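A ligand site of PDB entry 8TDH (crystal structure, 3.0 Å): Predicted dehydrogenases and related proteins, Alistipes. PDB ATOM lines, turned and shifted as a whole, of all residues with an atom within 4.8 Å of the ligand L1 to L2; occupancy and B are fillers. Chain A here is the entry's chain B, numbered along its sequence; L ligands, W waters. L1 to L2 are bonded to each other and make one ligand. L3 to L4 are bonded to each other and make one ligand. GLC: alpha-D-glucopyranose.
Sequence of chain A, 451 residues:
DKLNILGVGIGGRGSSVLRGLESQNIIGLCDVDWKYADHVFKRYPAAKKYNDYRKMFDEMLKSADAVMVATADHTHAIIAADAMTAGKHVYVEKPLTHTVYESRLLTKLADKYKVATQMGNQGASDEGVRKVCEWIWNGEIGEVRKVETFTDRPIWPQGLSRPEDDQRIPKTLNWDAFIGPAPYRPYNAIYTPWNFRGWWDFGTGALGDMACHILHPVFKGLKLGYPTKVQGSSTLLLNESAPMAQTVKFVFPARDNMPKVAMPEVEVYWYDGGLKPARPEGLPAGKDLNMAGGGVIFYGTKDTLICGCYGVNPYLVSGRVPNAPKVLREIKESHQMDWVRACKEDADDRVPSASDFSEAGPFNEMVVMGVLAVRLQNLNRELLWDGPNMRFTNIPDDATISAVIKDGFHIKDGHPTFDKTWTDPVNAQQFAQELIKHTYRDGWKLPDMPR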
ATOM      1  N   PRO A 183      12.713  15.872 -13.484  1.00  0.00           N
ATOM      2  CA  PRO A 183      12.383  16.709 -14.639  1.00  0.00           C
ATOM      3  C   PRO A 183      13.476  17.761 -14.785  1.00  0.00           C
ATOM      4  O   PRO A 183      13.963  18.286 -13.768  1.00  0.00           O
ATOM      5  CB  PRO A 183      11.033  17.342 -14.293  1.00  0.00           C
ATOM      6  CG  PRO A 183      10.583  16.606 -13.054  1.00  0.00           C
ATOM      7  CD  PRO A 183      11.835  16.138 -12.333  1.00  0.00           C
ATOM      8  N   ASP A 201      11.868  18.021  -5.966  1.00  0.00           N
ATOM      9  CA  ASP A 201      12.201  17.034  -6.986  1.00  0.00           C
ATOM     10  C   ASP A 201      13.574  16.408  -6.772  1.00  0.00           C
ATOM     11  O   ASP A 201      13.937  15.484  -7.458  1.00  0.00           O
ATOM     12  CB  ASP A 201      12.033  17.656  -8.367  1.00  0.00           C
ATOM     13  CG  ASP A 201      10.625  18.080  -8.789  1.00  0.00           C
ATOM     14  OD1 ASP A 201       9.687  17.867  -8.029  1.00  0.00           O
ATOM     15  OD2 ASP A 201      10.436  18.625  -9.923  1.00  0.00           O
ATOM     16  N   ASN A 239       4.884  24.611  -4.752  1.00  0.00           N
ATOM     17  CA  ASN A 239       4.788  23.543  -5.700  1.00  0.00           C
ATOM     18  C   ASN A 239       6.171  22.964  -5.946  1.00  0.00           C
ATOM     19  O   ASN A 239       6.275  21.810  -6.348  1.00  0.00           O
ATOM     20  CB  ASN A 239       4.068  23.965  -6.958  1.00  0.00           C
ATOM     21  CG  ASN A 239       4.888  24.852  -7.859  1.00  0.00           C
ATOM     22  OD1 ASN A 239       5.072  24.511  -9.029  1.00  0.00           O
ATOM     23  ND2 ASN A 239       5.406  25.973  -7.351  1.00  0.00           N
ATOM     24  N   GLU A 240       7.247  23.726  -5.695  1.00  0.00           N
ATOM     25  CA  GLU A 240       8.591  23.224  -5.980  1.00  0.00           C
ATOM     26  C   GLU A 240       9.468  23.115  -4.737  1.00  0.00           C
ATOM     27  O   GLU A 240      10.468  22.414  -4.813  1.00  0.00           O
ATOM     28  CB  GLU A 240       9.284  24.191  -6.929  1.00  0.00           C
ATOM     29  CG  GLU A 240       8.718  24.148  -8.350  1.00  0.00           C
ATOM     30  CD  GLU A 240       9.591  24.994  -9.260  1.00  0.00           C
ATOM     31  OE1 GLU A 240       9.233  26.199  -9.469  1.00  0.00           O
ATOM     32  OE2 GLU A 240      10.652  24.440  -9.735  1.00  0.00           O
ATOM     33  N   ARG A 375       2.081  17.140   1.256  1.00  0.00           N
ATOM     34  CA  ARG A 375       1.717  17.667  -0.056  1.00  0.00           C
ATOM     35  C   ARG A 375       0.260  17.347  -0.392  1.00  0.00           C
ATOM     36  O   ARG A 375      -0.361  18.051  -1.215  1.00  0.00           O
ATOM     37  CB  ARG A 375       2.638  17.129  -1.163  1.00  0.00           C
ATOM     38  CG  ARG A 375       4.044  17.723  -1.063  1.00  0.00           C
ATOM     39  CD  ARG A 375       5.089  17.325  -2.099  1.00  0.00           C
ATOM     40  NE  ARG A 375       4.984  18.151  -3.291  1.00  0.00           N
ATOM     41  CZ  ARG A 375       5.524  17.856  -4.457  1.00  0.00           C
ATOM     42  NH1 ARG A 375       6.279  16.774  -4.608  1.00  0.00           N
ATOM     43  NH2 ARG A 375       5.306  18.639  -5.488  1.00  0.00           N
ATOM     44  N   ILE A 401      -5.768  18.521  -7.068  1.00  0.00           N
ATOM     45  CA  ILE A 401      -4.749  19.098  -6.212  1.00  0.00           C
ATOM     46  C   ILE A 401      -4.210  20.345  -6.927  1.00  0.00           C
ATOM     47  O   ILE A 401      -4.026  20.348  -8.150  1.00  0.00           O
ATOM     48  CB  ILE A 401      -3.647  18.055  -5.968  1.00  0.00           C
ATOM     49  CG1 ILE A 401      -3.903  17.277  -4.744  1.00  0.00           C
ATOM     50  CG2 ILE A 401      -2.269  18.671  -5.846  1.00  0.00           C
ATOM     51  CD1 ILE A 401      -3.309  17.922  -3.504  1.00  0.00           C
ATOM     52  N   SER A 402      -3.883  21.360  -6.140  1.00  0.00           N
ATOM     53  CA  SER A 402      -3.285  22.584  -6.659  1.00  0.00           C
ATOM     54  C   SER A 402      -2.331  23.170  -5.614  1.00  0.00           C
ATOM     55  O   SER A 402      -2.685  23.273  -4.441  1.00  0.00           O
ATOM     56  CB  SER A 402      -4.377  23.536  -6.984  1.00  0.00           C
ATOM     57  OG  SER A 402      -3.903  24.468  -7.924  1.00  0.00           O
ATOM     58  N   ALA A 403      -1.128  23.543  -6.008  1.00  0.00           N
ATOM     59  CA  ALA A 403      -0.196  24.127  -5.051  1.00  0.00           C
ATOM     60  C   ALA A 403      -0.043  25.620  -5.308  1.00  0.00           C
ATOM     61  O   ALA A 403      -0.353  26.078  -6.395  1.00  0.00           O
ATOM     62  CB  ALA A 403       1.146  23.428  -5.129  1.00  0.00           C
ATOM     63  N   THR A 423      -0.804  26.621  -9.219  1.00  0.00           N
ATOM     64  CA  THR A 423      -0.575  25.724 -10.325  1.00  0.00           C
ATOM     65  C   THR A 423      -1.918  25.370 -10.982  1.00  0.00           C
ATOM     66  O   THR A 423      -2.984  25.660 -10.462  1.00  0.00           O
ATOM     67  CB  THR A 423       0.162  24.477  -9.842  1.00  0.00           C
ATOM     68  OG1 THR A 423      -0.605  23.955  -8.769  1.00  0.00           O
ATOM     69  CG2 THR A 423       1.543  24.719  -9.290  1.00  0.00           C
ATOM     70  N   ASP A 424      -1.850  24.757 -12.164  1.00  0.00           N
ATOM     71  CA  ASP A 424      -3.044  24.294 -12.860  1.00  0.00           C
ATOM     72  C   ASP A 424      -3.473  23.037 -12.124  1.00  0.00           C
ATOM     73  O   ASP A 424      -2.610  22.210 -11.807  1.00  0.00           O
ATOM     74  CB  ASP A 424      -2.796  24.049 -14.355  1.00  0.00           C
ATOM     75  CG  ASP A 424      -2.136  25.169 -15.197  1.00  0.00           C
ATOM     76  OD1 ASP A 424      -2.573  26.350 -15.085  1.00  0.00           O
ATOM     77  OD2 ASP A 424      -1.186  24.886 -16.014  1.00  0.00           O
ATOM     78  N   VAL A 426      -4.216  19.328 -11.130  1.00  0.00           N
ATOM     79  CA  VAL A 426      -4.034  17.981 -11.683  1.00  0.00           C
ATOM     80  C   VAL A 426      -4.841  16.991 -10.859  1.00  0.00           C
ATOM     81  O   VAL A 426      -5.237  17.262  -9.750  1.00  0.00           O
ATOM     82  CB  VAL A 426      -2.614  17.425 -11.814  1.00  0.00           C
ATOM     83  CG1 VAL A 426      -1.906  17.928 -13.099  1.00  0.00           C
ATOM     84  CG2 VAL A 426      -1.809  17.595 -10.519  1.00  0.00           C
ATOM     85  N   PHE A 431      -1.542  12.566  -9.173  1.00  0.00           N
ATOM     86  CA  PHE A 431      -0.518  13.347  -8.508  1.00  0.00           C
ATOM     87  C   PHE A 431       0.170  12.455  -7.488  1.00  0.00           C
ATOM     88  O   PHE A 431       1.394  12.395  -7.465  1.00  0.00           O
ATOM     89  CB  PHE A 431      -1.078  14.518  -7.710  1.00  0.00           C
ATOM     90  CG  PHE A 431      -0.083  15.372  -6.954  1.00  0.00           C
ATOM     91  CD1 PHE A 431       1.075  15.776  -7.562  1.00  0.00           C
ATOM     92  CD2 PHE A 431      -0.329  15.821  -5.674  1.00  0.00           C
ATOM     93  CE1 PHE A 431       1.948  16.646  -6.919  1.00  0.00           C
ATOM     94  CE2 PHE A 431       0.554  16.651  -5.019  1.00  0.00           C
ATOM     95  CZ  PHE A 431       1.686  17.093  -5.654  1.00  0.00           C
ATOM     96  N   LEU A 435       4.153  10.918  -6.905  1.00  0.00           N
ATOM     97  CA  LEU A 435       5.029  11.139  -5.760  1.00  0.00           C
ATOM     98  C   LEU A 435       5.507   9.819  -5.153  1.00  0.00           C
ATOM     99  O   LEU A 435       6.550   9.789  -4.510  1.00  0.00           O
ATOM    100  CB  LEU A 435       4.334  11.946  -4.653  1.00  0.00           C
ATOM    101  CG  LEU A 435       3.781  13.308  -5.050  1.00  0.00           C
ATOM    102  CD1 LEU A 435       3.355  14.047  -3.832  1.00  0.00           C
ATOM    103  CD2 LEU A 435       4.731  14.139  -5.875  1.00  0.00           C
ATOM    104  N   HIS A 438       7.936   7.879  -9.199  1.00  0.00           N
ATOM    105  CA  HIS A 438       8.172   8.933 -10.174  1.00  0.00           C
ATOM    106  C   HIS A 438       8.194   8.321 -11.566  1.00  0.00           C
ATOM    107  O   HIS A 438       8.562   7.160 -11.698  1.00  0.00           O
ATOM    108  CB  HIS A 438       9.500   9.642  -9.902  1.00  0.00           C
ATOM    109  CG  HIS A 438       9.438  10.561  -8.747  1.00  0.00           C
ATOM    110  ND1 HIS A 438      10.338  10.620  -7.705  1.00  0.00           N
ATOM    111  CD2 HIS A 438       8.523  11.525  -8.538  1.00  0.00           C
ATOM    112  CE1 HIS A 438       9.972  11.603  -6.896  1.00  0.00           C
ATOM    113  NE2 HIS A 438       8.873  12.147  -7.380  1.00  0.00           N
HETATM  114  C1  GLC L   1       2.513  18.723 -10.151  1.00  0.00           C
HETATM  115  C2  GLC L   1       2.362  18.133 -11.562  1.00  0.00           C
HETATM  116  C3  GLC L   1       1.622  19.100 -12.493  1.00  0.00           C
HETATM  117  C4  GLC L   1       0.476  19.888 -11.768  1.00  0.00           C
HETATM  118  C5  GLC L   1       0.939  20.396 -10.405  1.00  0.00           C
HETATM  119  C6  GLC L   1      -0.097  21.106  -9.561  1.00  0.00           C
HETATM  120  O1  GLC L   1       3.403  19.847 -10.024  1.00  0.00           O
HETATM  121  O2  GLC L   1       3.603  17.731 -12.155  1.00  0.00           O
HETATM  122  O3  GLC L   1       1.143  18.261 -13.568  1.00  0.00           O
HETATM  123  O4  GLC L   1      -0.004  20.998 -12.512  1.00  0.00           O
HETATM  124  O5  GLC L   1       1.273  19.223  -9.661  1.00  0.00           O
HETATM  125  O6  GLC L   1       0.349  21.318  -8.177  1.00  0.00           O
HETATM  126  C1  GLC L   2       4.382  19.751  -9.060  1.00  0.00           C
HETATM  127  C2  GLC L   2       5.383  20.854  -9.257  1.00  0.00           C
HETATM  128  C3  GLC L   2       6.579  20.600 -10.180  1.00  0.00           C
HETATM  129  C4  GLC L   2       7.240  19.219 -10.045  1.00  0.00           C
HETATM  130  C5  GLC L   2       6.278  18.110  -9.499  1.00  0.00           C
HETATM  131  C6  GLC L   2       6.689  17.605  -8.154  1.00  0.00           C
HETATM  132  O2  GLC L   2       4.555  21.920  -9.703  1.00  0.00           O
HETATM  133  O3  GLC L   2       7.602  21.538  -9.881  1.00  0.00           O
HETATM  134  O4  GLC L   2       7.794  18.735 -11.321  1.00  0.00           O
HETATM  135  O5  GLC L   2       4.897  18.434  -9.263  1.00  0.00           O
HETATM  136  O6  GLC L   2       7.180  16.283  -8.351  1.00  0.00           O
HETATM  137  C1  GLC L   3       3.176  13.483 -13.895  1.00  0.00           C
HETATM  138  C2  GLC L   3       3.097  12.167 -14.666  1.00  0.00           C
HETATM  139  C3  GLC L   3       1.732  12.103 -15.352  1.00  0.00           C
HETATM  140  C4  GLC L   3       0.635  12.288 -14.317  1.00  0.00           C
HETATM  141  C5  GLC L   3       0.809  13.638 -13.596  1.00  0.00           C
HETATM  142  C6  GLC L   3      -0.253  13.933 -12.557  1.00  0.00           C
HETATM  143  O1  GLC L   3       3.136  14.503 -14.832  1.00  0.00           O
HETATM  144  O2  GLC L   3       4.202  11.948 -15.565  1.00  0.00           O
HETATM  145  O3  GLC L   3       1.542  10.856 -16.020  1.00  0.00           O
HETATM  146  O4  GLC L   3      -0.617  12.220 -14.967  1.00  0.00           O
HETATM  147  O5  GLC L   3       2.105  13.632 -12.952  1.00  0.00           O
HETATM  148  O6  GLC L   3       0.044  15.165 -11.885  1.00  0.00           O
HETATM  149  C1  GLC L   4       4.126  15.458 -14.851  1.00  0.00           C
HETATM  150  C2  GLC L   4       3.650  16.603 -15.788  1.00  0.00           C
HETATM  151  C3  GLC L   4       4.379  16.528 -17.135  1.00  0.00           C
HETATM  152  C4  GLC L   4       5.900  16.482 -16.980  1.00  0.00           C
HETATM  153  C5  GLC L   4       6.421  15.581 -15.783  1.00  0.00           C
HETATM  154  C6  GLC L   4       7.074  16.397 -14.663  1.00  0.00           C
HETATM  155  O2  GLC L   4       2.221  16.589 -15.945  1.00  0.00           O
HETATM  156  O3  GLC L   4       4.073  17.660 -17.937  1.00  0.00           O
HETATM  157  O4  GLC L   4       6.466  15.997 -18.194  1.00  0.00           O
HETATM  158  O5  GLC L   4       5.393  14.805 -15.136  1.00  0.00           O
HETATM  159  O6  GLC L   4       7.804  17.519 -15.183  1.00  0.00           O
HETATM  160  O   HOH W   1       6.553  13.612  -8.478  1.00  0.00           O
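The backbone NH of Ala 403 sits at hydrogen-bond distance from an oxygen (O6) of GLC L1, 3.4 Å away.
The side-chain hydroxyl (OG1) of Thr 423 is in hydrogen-bond range of an oxygen (O6) of GLC L1 (2.9 Å).
The side-chain carboxylate (OD1) of Asp 201 is in hydrogen-bond range of an oxygen (O6) of GLC L2, 3.0 Å away.
O2 of GLC L2 lies within hydrogen-bond range of OD1 of Asn 239 (2.7 Å).
O of Asp 424 is in hydrogen-bond range of O4 of GLC L1 (3.0 Å).
An oxygen (O3) of GLC L1 is in hydrogen-bond range of an oxygen (O2) of GLC L4.
The backbone carbonyl oxygen of Asn 239 lies within hydrogen-bond range of the guanidinium group of Arg 375 (3.4 Å).
The side-chain hydroxyl of Thr 423 is in hydrogen-bond range of the backbone NH of Ala 403 (2.8 Å).
The backbone NH (N) of Ile 401 sits at hydrogen-bond distance from the backbone carbonyl oxygen (O) of Val 426.
The side-chain hydroxyl (OG) of Ser 402 lies within hydrogen-bond range of the backbone carbonyl oxygen (O) of Thr 423 (3.0 Å).
Pro 183 touches the ligand L1 to L2.
CG of Glu 240 touches O3 of GLC L2, 3.2 Å away.
Arg 375 touches the ligand L1 to L2.
Val 426 touches the ligand L1 to L2.
CE1 of Phe 431 touches O5 of GLC L1, 3.8 Å away.
Hydrophobic or aromatic side chains within 4 Å of the ligand L1 to L2: Pro 183, Ala 403, Val 426 and Phe 431.
Of the 14 residues printed, 10 come within 4 Å of the ligand L1 to L2.
Along chain A the residues within 4 Å of the ligand L1 to L2 span positions 183 to 431.
Water W1 bridges O6 of GLC L2 and NE2 of His 438.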
